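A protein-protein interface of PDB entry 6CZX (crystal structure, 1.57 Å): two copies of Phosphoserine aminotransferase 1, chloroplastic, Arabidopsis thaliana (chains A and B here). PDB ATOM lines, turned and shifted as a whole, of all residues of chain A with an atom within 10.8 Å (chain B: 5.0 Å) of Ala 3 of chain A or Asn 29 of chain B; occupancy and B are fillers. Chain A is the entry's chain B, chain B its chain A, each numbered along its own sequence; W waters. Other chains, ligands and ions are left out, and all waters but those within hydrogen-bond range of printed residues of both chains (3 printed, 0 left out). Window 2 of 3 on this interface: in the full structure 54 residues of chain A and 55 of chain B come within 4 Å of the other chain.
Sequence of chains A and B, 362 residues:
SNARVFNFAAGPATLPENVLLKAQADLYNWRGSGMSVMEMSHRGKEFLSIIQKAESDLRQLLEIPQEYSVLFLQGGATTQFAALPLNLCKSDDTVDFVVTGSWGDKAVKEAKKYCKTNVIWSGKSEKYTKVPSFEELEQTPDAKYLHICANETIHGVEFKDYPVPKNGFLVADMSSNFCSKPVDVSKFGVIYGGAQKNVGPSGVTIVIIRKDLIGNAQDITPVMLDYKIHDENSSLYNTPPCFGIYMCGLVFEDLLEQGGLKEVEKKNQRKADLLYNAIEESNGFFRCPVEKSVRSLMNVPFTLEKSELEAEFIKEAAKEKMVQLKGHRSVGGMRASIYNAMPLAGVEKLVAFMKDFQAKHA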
ATOM      1  N   ASN A   2      -5.704  13.247  10.543  1.00  0.00           N
ATOM      2  CA  ASN A   2      -6.198  13.488  11.953  1.00  0.00           C
ATOM      3  C   ASN A   2      -7.530  14.278  12.014  1.00  0.00           C
ATOM      4  O   ASN A   2      -7.705  15.172  12.833  1.00  0.00           O
ATOM      5  CB  ASN A   2      -5.100  14.194  12.772  1.00  0.00           C
ATOM      6  CG  ASN A   2      -3.831  13.346  12.908  1.00  0.00           C
ATOM      7  OD1 ASN A   2      -3.894  12.110  13.033  1.00  0.00           O
ATOM      8  ND2 ASN A   2      -2.676  14.002  12.865  1.00  0.00           N
ATOM      9  N   ALA A   3      -8.452  13.975  11.108  1.00  0.00           N
ATOM     10  CA  ALA A   3      -9.784  14.534  11.154  1.00  0.00           C
ATOM     11  C   ALA A   3     -10.604  13.699  12.155  1.00  0.00           C
ATOM     12  O   ALA A   3     -10.259  12.531  12.464  1.00  0.00           O
ATOM     13  CB  ALA A   3     -10.449  14.467   9.780  1.00  0.00           C
ATOM     14  N   ARG A   4     -11.707  14.279  12.614  1.00  0.00           N
ATOM     15  CA  ARG A   4     -12.604  13.512  13.464  1.00  0.00           C
ATOM     16  C   ARG A   4     -13.291  12.441  12.644  1.00  0.00           C
ATOM     17  O   ARG A   4     -13.594  12.620  11.440  1.00  0.00           O
ATOM     18  CB  ARG A   4     -13.616  14.371  14.176  1.00  0.00           C
ATOM     19  CG  ARG A   4     -12.935  15.060  15.363  1.00  0.00           C
ATOM     20  CD  ARG A   4     -13.793  16.090  16.022  1.00  0.00           C
ATOM     21  NE  ARG A   4     -15.131  15.607  16.319  1.00  0.00           N
ATOM     22  CZ  ARG A   4     -15.502  15.036  17.456  1.00  0.00           C
ATOM     23  NH1 ARG A   4     -14.644  14.816  18.451  1.00  0.00           N
ATOM     24  NH2 ARG A   4     -16.757  14.654  17.591  1.00  0.00           N
ATOM     25  N   VAL A   5     -13.487  11.305  13.267  1.00  0.00           N
ATOM     26  CA  VAL A   5     -14.175  10.195  12.632  1.00  0.00           C
ATOM     27  C   VAL A   5     -15.686  10.194  12.891  1.00  0.00           C
ATOM     28  O   VAL A   5     -16.197  10.894  13.782  1.00  0.00           O
ATOM     29  CB  VAL A   5     -13.593   8.825  13.089  1.00  0.00           C
ATOM     30  CG1 VAL A   5     -12.111   8.700  12.729  1.00  0.00           C
ATOM     31  CG2 VAL A   5     -13.761   8.592  14.582  1.00  0.00           C
ATOM     32  N   PHE A   6     -16.407   9.400  12.111  1.00  0.00           N
ATOM     33  CA  PHE A   6     -17.786   9.090  12.422  1.00  0.00           C
ATOM     34  C   PHE A   6     -17.805   7.955  13.421  1.00  0.00           C
ATOM     35  O   PHE A   6     -17.407   6.845  13.122  1.00  0.00           O
ATOM     36  CB  PHE A   6     -18.593   8.729  11.182  1.00  0.00           C
ATOM     37  CG  PHE A   6     -18.756   9.864  10.207  1.00  0.00           C
ATOM     38  CD1 PHE A   6     -19.447  11.022  10.579  1.00  0.00           C
ATOM     39  CD2 PHE A   6     -18.215   9.778   8.941  1.00  0.00           C
ATOM     40  CE1 PHE A   6     -19.603  12.079   9.698  1.00  0.00           C
ATOM     41  CE2 PHE A   6     -18.371  10.828   8.053  1.00  0.00           C
ATOM     42  CZ  PHE A   6     -19.057  11.971   8.442  1.00  0.00           C
ATOM     43  N   ASN A   7     -18.335   8.235  14.615  1.00  0.00           N
ATOM     44  CA  ASN A   7     -18.153   7.389  15.767  1.00  0.00           C
ATOM     45  C   ASN A   7     -19.480   6.737  16.124  1.00  0.00           C
ATOM     46  O   ASN A   7     -20.354   7.361  16.745  1.00  0.00           O
ATOM     47  CB  ASN A   7     -17.642   8.246  16.908  1.00  0.00           C
ATOM     48  CG  ASN A   7     -17.452   7.497  18.203  1.00  0.00           C
ATOM     49  OD1 ASN A   7     -17.568   6.259  18.279  1.00  0.00           O
ATOM     50  ND2 ASN A   7     -17.228   8.267  19.263  1.00  0.00           N
ATOM     51  N   LEU A  15     -20.451  13.219  20.669  1.00  0.00           N
ATOM     52  CA  LEU A  15     -21.010  14.423  21.237  1.00  0.00           C
ATOM     53  C   LEU A  15     -20.994  15.556  20.190  1.00  0.00           C
ATOM     54  O   LEU A  15     -20.234  15.494  19.233  1.00  0.00           O
ATOM     55  CB  LEU A  15     -20.250  14.850  22.485  1.00  0.00           C
ATOM     56  CG  LEU A  15     -20.465  13.957  23.708  1.00  0.00           C
ATOM     57  CD1 LEU A  15     -19.424  14.233  24.775  1.00  0.00           C
ATOM     58  CD2 LEU A  15     -21.858  14.173  24.268  1.00  0.00           C
ATOM     59  N   PRO A  16     -21.858  16.567  20.365  1.00  0.00           N
ATOM     60  CA  PRO A  16     -21.868  17.652  19.377  1.00  0.00           C
ATOM     61  C   PRO A  16     -20.531  18.396  19.353  1.00  0.00           C
ATOM     62  O   PRO A  16     -19.956  18.662  20.408  1.00  0.00           O
ATOM     63  CB  PRO A  16     -22.975  18.563  19.855  1.00  0.00           C
ATOM     64  CG  PRO A  16     -23.835  17.732  20.734  1.00  0.00           C
ATOM     65  CD  PRO A  16     -22.885  16.755  21.402  1.00  0.00           C
ATOM     66  N   GLU A  17     -20.001  18.654  18.162  1.00  0.00           N
ATOM     67  CA  GLU A  17     -18.726  19.350  18.039  1.00  0.00           C
ATOM     68  C   GLU A  17     -18.767  20.755  18.652  1.00  0.00           C
ATOM     69  O   GLU A  17     -17.808  21.154  19.308  1.00  0.00           O
ATOM     70  CB  GLU A  17     -18.210  19.381  16.588  1.00  0.00           C
ATOM     71  CG  GLU A  17     -17.854  17.993  16.101  1.00  0.00           C
ATOM     72  CD  GLU A  17     -17.432  17.899  14.652  1.00  0.00           C
ATOM     73  OE1 GLU A  17     -17.701  18.838  13.839  1.00  0.00           O
ATOM     74  OE2 GLU A  17     -16.817  16.871  14.312  1.00  0.00           O
ATOM     75  N   LEU A  20     -18.298  20.292  22.359  1.00  0.00           N
ATOM     76  CA  LEU A  20     -16.914  19.971  22.708  1.00  0.00           C
ATOM     77  C   LEU A  20     -15.998  21.236  22.656  1.00  0.00           C
ATOM     78  O   LEU A  20     -15.121  21.447  23.512  1.00  0.00           O
ATOM     79  CB  LEU A  20     -16.358  18.904  21.770  1.00  0.00           C
ATOM     80  CG  LEU A  20     -17.001  17.535  21.880  1.00  0.00           C
ATOM     81  CD1 LEU A  20     -16.534  16.646  20.740  1.00  0.00           C
ATOM     82  CD2 LEU A  20     -16.691  16.921  23.250  1.00  0.00           C
ATOM     83  N   LEU A  21     -16.205  22.040  21.632  1.00  0.00           N
ATOM     84  CA  LEU A  21     -15.413  23.254  21.448  1.00  0.00           C
ATOM     85  C   LEU A  21     -15.712  24.309  22.534  1.00  0.00           C
ATOM     86  O   LEU A  21     -14.830  25.016  22.998  1.00  0.00           O
ATOM     87  CB  LEU A  21     -15.585  23.785  20.008  1.00  0.00           C
ATOM     88  CG  LEU A  21     -14.938  22.837  18.989  1.00  0.00           C
ATOM     89  CD1 LEU A  21     -15.380  23.170  17.579  1.00  0.00           C
ATOM     90  CD2 LEU A  21     -13.430  22.839  19.065  1.00  0.00           C
ATOM     91  N   GLN A  24     -13.869  23.109  25.479  1.00  0.00           N
ATOM     92  CA  GLN A  24     -12.455  23.365  25.329  1.00  0.00           C
ATOM     93  C   GLN A  24     -12.142  24.827  25.698  1.00  0.00           C
ATOM     94  O   GLN A  24     -11.163  25.130  26.377  1.00  0.00           O
ATOM     95  CB  GLN A  24     -12.032  23.084  23.879  1.00  0.00           C
ATOM     96  CG  GLN A  24     -10.567  23.342  23.597  1.00  0.00           C
ATOM     97  CD  GLN A  24     -10.243  23.050  22.144  1.00  0.00           C
ATOM     98  OE1 GLN A  24     -10.747  23.718  21.258  1.00  0.00           O
ATOM     99  NE2 GLN A  24      -9.397  22.046  21.882  1.00  0.00           N
ATOM    100  N   ALA A 318     -14.044   1.170   8.954  1.00  0.00           N
ATOM    101  CA  ALA A 318     -13.111   1.896   9.817  1.00  0.00           C
ATOM    102  C   ALA A 318     -12.034   2.620   8.998  1.00  0.00           C
ATOM    103  O   ALA A 318     -11.647   3.733   9.313  1.00  0.00           O
ATOM    104  CB  ALA A 318     -12.474   0.947  10.827  1.00  0.00           C
ATOM    105  N   LYS A 319     -11.595   2.012   7.904  1.00  0.00           N
ATOM    106  CA  LYS A 319     -10.662   2.705   7.003  1.00  0.00           C
ATOM    107  C   LYS A 319     -11.269   3.910   6.364  1.00  0.00           C
ATOM    108  O   LYS A 319     -10.545   4.838   6.002  1.00  0.00           O
ATOM    109  CB  LYS A 319     -10.171   1.799   5.877  1.00  0.00           C
ATOM    110  CG  LYS A 319      -9.387   0.601   6.347  1.00  0.00           C
ATOM    111  CD  LYS A 319      -8.779  -0.103   5.132  1.00  0.00           C
ATOM    112  CE  LYS A 319      -8.289  -1.474   5.518  1.00  0.00           C
ATOM    113  NZ  LYS A 319      -7.777  -2.168   4.315  1.00  0.00           N
ATOM    114  N   GLU A 320     -12.590   3.882   6.189  1.00  0.00           N
ATOM    115  CA  GLU A 320     -13.345   5.015   5.698  1.00  0.00           C
ATOM    116  C   GLU A 320     -13.910   5.916   6.844  1.00  0.00           C
ATOM    117  O   GLU A 320     -14.865   6.650   6.650  1.00  0.00           O
ATOM    118  CB  GLU A 320     -14.467   4.513   4.798  1.00  0.00           C
ATOM    119  CG  GLU A 320     -14.044   4.090   3.398  1.00  0.00           C
ATOM    120  CD  GLU A 320     -14.959   4.761   2.374  1.00  0.00           C
ATOM    121  OE1 GLU A 320     -14.596   5.884   1.922  1.00  0.00           O
ATOM    122  OE2 GLU A 320     -16.079   4.225   2.101  1.00  0.00           O
ATOM    123  N   LYS A 321     -13.288   5.854   8.017  1.00  0.00           N
ATOM    124  CA  LYS A 321     -13.559   6.772   9.136  1.00  0.00           C
ATOM    125  C   LYS A 321     -14.937   6.524   9.753  1.00  0.00           C
ATOM    126  O   LYS A 321     -15.546   7.443  10.307  1.00  0.00           O
ATOM    127  CB  LYS A 321     -13.451   8.251   8.726  1.00  0.00           C
ATOM    128  CG  LYS A 321     -12.196   8.652   7.977  1.00  0.00           C
ATOM    129  CD  LYS A 321     -10.961   8.566   8.856  1.00  0.00           C
ATOM    130  CE  LYS A 321      -9.987   7.514   8.375  1.00  0.00           C
ATOM    131  NZ  LYS A 321      -8.809   7.330   9.277  1.00  0.00           N
ATOM    132  N   MET A 322     -15.411   5.285   9.651  1.00  0.00           N
ATOM    133  CA  MET A 322     -16.671   4.885  10.324  1.00  0.00           C
ATOM    134  C   MET A 322     -16.329   3.772  11.298  1.00  0.00           C
ATOM    135  O   MET A 322     -16.099   2.631  10.893  1.00  0.00           O
ATOM    136  CB  MET A 322     -17.707   4.435   9.309  1.00  0.00           C
ATOM    137  CG  MET A 322     -18.196   5.569   8.438  1.00  0.00           C
ATOM    138  SD  MET A 322     -19.240   5.040   7.064  1.00  0.00           S
ATOM    139  CE  MET A 322     -18.078   4.162   6.034  1.00  0.00           C
ATOM    140  N   VAL A 323     -16.261   4.121  12.583  1.00  0.00           N
ATOM    141  CA  VAL A 323     -15.676   3.232  13.590  1.00  0.00           C
ATOM    142  C   VAL A 323     -16.709   2.747  14.605  1.00  0.00           C
ATOM    143  O   VAL A 323     -17.752   3.384  14.801  1.00  0.00           O
ATOM    144  CB  VAL A 323     -14.517   3.891  14.356  1.00  0.00           C
ATOM    145  CG1 VAL A 323     -13.414   4.307  13.385  1.00  0.00           C
ATOM    146  CG2 VAL A 323     -14.983   5.071  15.170  1.00  0.00           C
ATOM    147  N   LYS A 349     -22.877   8.476   4.763  1.00  0.00           N
ATOM    148  CA  LYS A 349     -21.659   7.797   4.384  1.00  0.00           C
ATOM    149  C   LYS A 349     -21.754   6.284   4.584  1.00  0.00           C
ATOM    150  O   LYS A 349     -21.298   5.510   3.750  1.00  0.00           O
ATOM    151  CB  LYS A 349     -20.456   8.367   5.128  1.00  0.00           C
ATOM    152  CG  LYS A 349     -19.144   7.880   4.526  1.00  0.00           C
ATOM    153  CD  LYS A 349     -17.933   8.522   5.149  1.00  0.00           C
ATOM    154  CE  LYS A 349     -16.709   8.203   4.321  1.00  0.00           C
ATOM    155  NZ  LYS A 349     -15.522   8.708   5.058  1.00  0.00           N
ATOM    156  N   ASP B  26      -6.094  18.598  23.889  1.00  0.00           N
ATOM    157  CA  ASP B  26      -6.491  17.310  23.325  1.00  0.00           C
ATOM    158  C   ASP B  26      -8.004  17.064  23.363  1.00  0.00           C
ATOM    159  O   ASP B  26      -8.467  15.977  22.999  1.00  0.00           O
ATOM    160  CB  ASP B  26      -5.736  16.188  24.056  1.00  0.00           C
ATOM    161  CG  ASP B  26      -4.261  16.164  23.685  1.00  0.00           C
ATOM    162  OD1 ASP B  26      -3.861  16.900  22.737  1.00  0.00           O
ATOM    163  OD2 ASP B  26      -3.450  15.456  24.336  1.00  0.00           O
ATOM    164  N   LEU B  27      -8.794  18.054  23.793  1.00  0.00           N
ATOM    165  CA  LEU B  27     -10.219  17.777  24.128  1.00  0.00           C
ATOM    166  C   LEU B  27     -11.058  17.378  22.919  1.00  0.00           C
ATOM    167  O   LEU B  27     -12.015  16.591  23.038  1.00  0.00           O
ATOM    168  CB  LEU B  27     -10.890  18.981  24.814  1.00  0.00           C
ATOM    169  CG  LEU B  27     -12.101  18.637  25.696  1.00  0.00           C
ATOM    170  CD1 LEU B  27     -11.691  17.839  26.908  1.00  0.00           C
ATOM    171  CD2 LEU B  27     -12.815  19.927  26.095  1.00  0.00           C
ATOM    172  N   TYR B  28     -10.743  17.940  21.767  1.00  0.00           N
ATOM    173  CA  TYR B  28     -11.553  17.725  20.552  1.00  0.00           C
ATOM    174  C   TYR B  28     -11.190  16.472  19.804  1.00  0.00           C
ATOM    175  O   TYR B  28     -12.031  15.873  19.097  1.00  0.00           O
ATOM    176  CB  TYR B  28     -11.365  18.900  19.612  1.00  0.00           C
ATOM    177  CG  TYR B  28     -12.327  19.023  18.483  1.00  0.00           C
ATOM    178  CD1 TYR B  28     -13.662  19.183  18.722  1.00  0.00           C
ATOM    179  CD2 TYR B  28     -11.880  19.094  17.173  1.00  0.00           C
ATOM    180  CE1 TYR B  28     -14.563  19.367  17.687  1.00  0.00           C
ATOM    181  CE2 TYR B  28     -12.780  19.276  16.131  1.00  0.00           C
ATOM    182  CZ  TYR B  28     -14.122  19.420  16.411  1.00  0.00           C
ATOM    183  OH  TYR B  28     -15.067  19.590  15.414  1.00  0.00           O
ATOM    184  N   ASN B  29      -9.927  16.090  19.928  1.00  0.00           N
ATOM    185  CA  ASN B  29      -9.353  14.960  19.167  1.00  0.00           C
ATOM    186  C   ASN B  29      -8.100  14.516  19.883  1.00  0.00           C
ATOM    187  O   ASN B  29      -7.046  15.143  19.748  1.00  0.00           O
ATOM    188  CB  ASN B  29      -9.071  15.379  17.716  1.00  0.00           C
ATOM    189  CG  ASN B  29      -8.623  14.229  16.838  1.00  0.00           C
ATOM    190  OD1 ASN B  29      -8.141  13.195  17.331  1.00  0.00           O
ATOM    191  ND2 ASN B  29      -8.782  14.407  15.480  1.00  0.00           N
ATOM    192  N   TRP B  30      -8.210  13.461  20.658  1.00  0.00           N
ATOM    193  CA  TRP B  30      -7.102  12.951  21.494  1.00  0.00           C
ATOM    194  C   TRP B  30      -6.107  12.179  20.633  1.00  0.00           C
ATOM    195  O   TRP B  30      -6.451  11.136  20.099  1.00  0.00           O
ATOM    196  CB  TRP B  30      -7.628  12.046  22.605  1.00  0.00           C
ATOM    197  CG  TRP B  30      -6.625  11.544  23.556  1.00  0.00           C
ATOM    198  CD1 TRP B  30      -6.120  12.203  24.635  1.00  0.00           C
ATOM    199  CD2 TRP B  30      -6.051  10.245  23.586  1.00  0.00           C
ATOM    200  NE1 TRP B  30      -5.252  11.410  25.309  1.00  0.00           N
ATOM    201  CE2 TRP B  30      -5.180  10.199  24.675  1.00  0.00           C
ATOM    202  CE3 TRP B  30      -6.168   9.129  22.779  1.00  0.00           C
ATOM    203  CZ2 TRP B  30      -4.442   9.055  24.991  1.00  0.00           C
ATOM    204  CZ3 TRP B  30      -5.434   8.021  23.059  1.00  0.00           C
ATOM    205  CH2 TRP B  30      -4.593   7.969  24.169  1.00  0.00           C
ATOM    206  N   ARG B  31      -4.879  12.690  20.508  1.00  0.00           N
ATOM    207  CA  ARG B  31      -3.810  11.958  19.805  1.00  0.00           C
ATOM    208  C   ARG B  31      -4.190  11.381  18.425  1.00  0.00           C
ATOM    209  O   ARG B  31      -3.948  10.189  18.150  1.00  0.00           O
ATOM    210  CB  ARG B  31      -3.343  10.805  20.664  1.00  0.00           C
ATOM    211  CG  ARG B  31      -2.660  11.215  21.941  1.00  0.00           C
ATOM    212  CD  ARG B  31      -1.852  10.069  22.485  1.00  0.00           C
ATOM    213  NE  ARG B  31      -1.335  10.423  23.794  1.00  0.00           N
ATOM    214  CZ  ARG B  31      -0.907   9.561  24.728  1.00  0.00           C
ATOM    215  NH1 ARG B  31      -0.457   9.984  25.902  1.00  0.00           N
ATOM    216  NH2 ARG B  31      -0.964   8.259  24.496  1.00  0.00           N
ATOM    217  N   GLY B  32      -4.821  12.171  17.580  1.00  0.00           N
ATOM    218  CA  GLY B  32      -5.315  11.681  16.267  1.00  0.00           C
ATOM    219  C   GLY B  32      -6.198  10.424  16.249  1.00  0.00           C
ATOM    220  O   GLY B  32      -6.317   9.758  15.220  1.00  0.00           O
ATOM    221  N   SER B  33      -6.816  10.080  17.373  1.00  0.00           N
ATOM    222  CA  SER B  33      -7.782   8.988  17.411  1.00  0.00           C
ATOM    223  C   SER B  33      -9.072   9.353  16.704  1.00  0.00           C
ATOM    224  O   SER B  33      -9.916   8.505  16.445  1.00  0.00           O
ATOM    225  CB  SER B  33      -8.122   8.636  18.843  1.00  0.00           C
ATOM    226  OG  SER B  33      -8.827   9.680  19.485  1.00  0.00           O
ATOM    227  N   GLY B  34      -9.296  10.639  16.511  1.00  0.00           N
ATOM    228  CA  GLY B  34     -10.484  11.087  15.819  1.00  0.00           C
ATOM    229  C   GLY B  34     -11.685  11.382  16.719  1.00  0.00           C
ATOM    230  O   GLY B  34     -12.760  11.658  16.205  1.00  0.00           O
ATOM    231  N   MET B  35     -11.453  11.466  18.022  1.00  0.00           N
ATOM    232  CA  MET B  35     -12.522  11.776  18.974  1.00  0.00           C
ATOM    233  C   MET B  35     -11.970  12.255  20.304  1.00  0.00           C
ATOM    234  O   MET B  35     -10.761  12.122  20.610  1.00  0.00           O
ATOM    235  CB  MET B  35     -13.396  10.535  19.184  1.00  0.00           C
ATOM    236  CG  MET B  35     -12.664   9.422  19.933  1.00  0.00           C
ATOM    237  SD  MET B  35     -13.641   7.895  20.002  1.00  0.00           S
ATOM    238  CE  MET B  35     -13.710   7.369  18.313  1.00  0.00           C
ATOM    239  N   SER B  36     -12.857  12.824  21.128  1.00  0.00           N
ATOM    240  CA  SER B  36     -12.501  13.241  22.476  1.00  0.00           C
ATOM    241  C   SER B  36     -12.427  12.023  23.383  1.00  0.00           C
ATOM    242  O   SER B  36     -13.148  11.031  23.165  1.00  0.00           O
ATOM    243  CB  SER B  36     -13.626  14.132  23.017  1.00  0.00           C
ATOM    244  OG  SER B  36     -13.391  14.560  24.338  1.00  0.00           O
HETATM  245  O   HOH W   1      -9.336  17.229  14.580  1.00  0.00           O
HETATM  246  O   HOH W   2     -15.886   5.248  20.359  1.00  0.00           O
HETATM  247  O   HOH W   3     -15.425  11.558  16.385  1.00  0.00           O
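OD1 of Asn 29 of chain B is in hydrogen-bond range of N of Ser 33 of chain B (3.4 Å).
The guanidinium group of Arg 4 of chain A is in salt-bridge range of the side-chain carboxylate of Glu 17 of chain A, 2.9 Å away.
The backbone carbonyl oxygen of Leu 27 of chain B lies within hydrogen-bond range of the side-chain hydroxyl of Ser 36 of chain B, at 2.8 Å.
The side-chain amide oxygen (OD1) of Asn 29 of chain B lies within hydrogen-bond range of the backbone NH (N) of Gly 34 of chain B (2.9 Å).
The backbone NH (N) of Gly 32 of chain B sits close to the side-chain amide oxygen (OD1) of Asn 29 of chain B (3.5 Å).
The backbone NH (N) of Trp 30 of chain B sits at hydrogen-bond distance from the backbone carbonyl oxygen (O) of Met 35 of chain B, 2.9 Å away.
Water W3 bridges O of Gly 34 of chain B (2.7 Å) and O of Val 5 of chain A (2.8 Å).
Water W2 bridges OD1 of Asn 7 of chain A (2.9 Å) and SD of Met 35 of chain B (3.5 Å).
Water W1 lies within hydrogen-bond range of the side-chain amide nitrogen of Asn 29 of chain B (3.0 Å) and the backbone carbonyl oxygen of Asn 2 of chain A (3.2 Å).
ND2 of Asn 29 of chain B sits at hydrogen-bond distance from O of Asn 2 of chain A (3.0 Å).
The backbone NH (N) of Val 5 of chain A lies within hydrogen-bond range of the backbone carbonyl oxygen (O) of Gly 34 of chain B.
NH1 of Arg 4 of chain A sits at hydrogen-bond distance from O of Tyr 28 of chain B.
The side-chain hydroxyl (OH) of Tyr 28 of chain B sits close to the side-chain carboxylate (OE1) of Glu 17 of chain A, at 3.2 Å.
The side-chain sulfur of Met 35 of chain B sits at hydrogen-bond distance from the side-chain amide nitrogen of Asn 7 of chain A (3.7 Å).
Of the 11 printed residues of chain B, 7 touch a printed residue of chain A.
Printed residues of chain B that touch a printed residue of chain A: Leu 27, Tyr 28, Asn 29, Gly 32, Gly 34, Met 35 and Ser 36.
Hydrophobic or aromatic side chains of chain B within 4 Å of the printed part of chain A: Leu 27, Tyr 28 and Met 35.
Along chain B the printed residues that touch a printed residue of chain A span positions 27 to 36.
Among the printed residues, 15 pairs touch across the chains.
No position is printed for both chains.
Ala 3 of chain A touches two residues of chain B.
Asn 29 of chain B touches two residues of chain A.
Gly 32 of chain B touches just one residue of chain A: Asn 2 (3.6 Å).
Of the printed residues of chain B, Leu 21 of chain A touches Tyr 28 (3.7 Å).
Of the printed residues of chain B, Asn 7 of chain A touches Met 35.
Glu 320 of chain A touches none of the printed residues of chain B.
The nearest printed residue of chain B that does not touch Ala 3 of chain A is Ser 33 of chain B (5.4 Å).
The nearest residue of chain A that does not touch Asn 29 of chain B is Arg 4 of chain A (4.1 Å).
Among the printed residues, pairs that only touch across the chains: Arg 4 of chain A with Gly 34 of chain B (3.3 Å), Gln 24 of chain A with Leu 27 of chain B (3.4 Å), Asn 2 of chain A with Gly 32 of chain B (3.6 Å), Ala 3 of chain A with Gly 34 of chain B (3.7 Å), Leu 21 of chain A with Tyr 28 of chain B (3.7 Å), Arg 4 of chain A with Met 35 of chain B (3.7 Å), Leu 20 of chain A with Leu 27 of chain B (3.8 Å), Arg 4 of chain A with Ser 36 of chain B (3.8 Å), Ala 3 of chain A with Asn 29 of chain B (3.8 Å) and Val 5 of chain A with Met 35 of chain B (3.9 Å).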
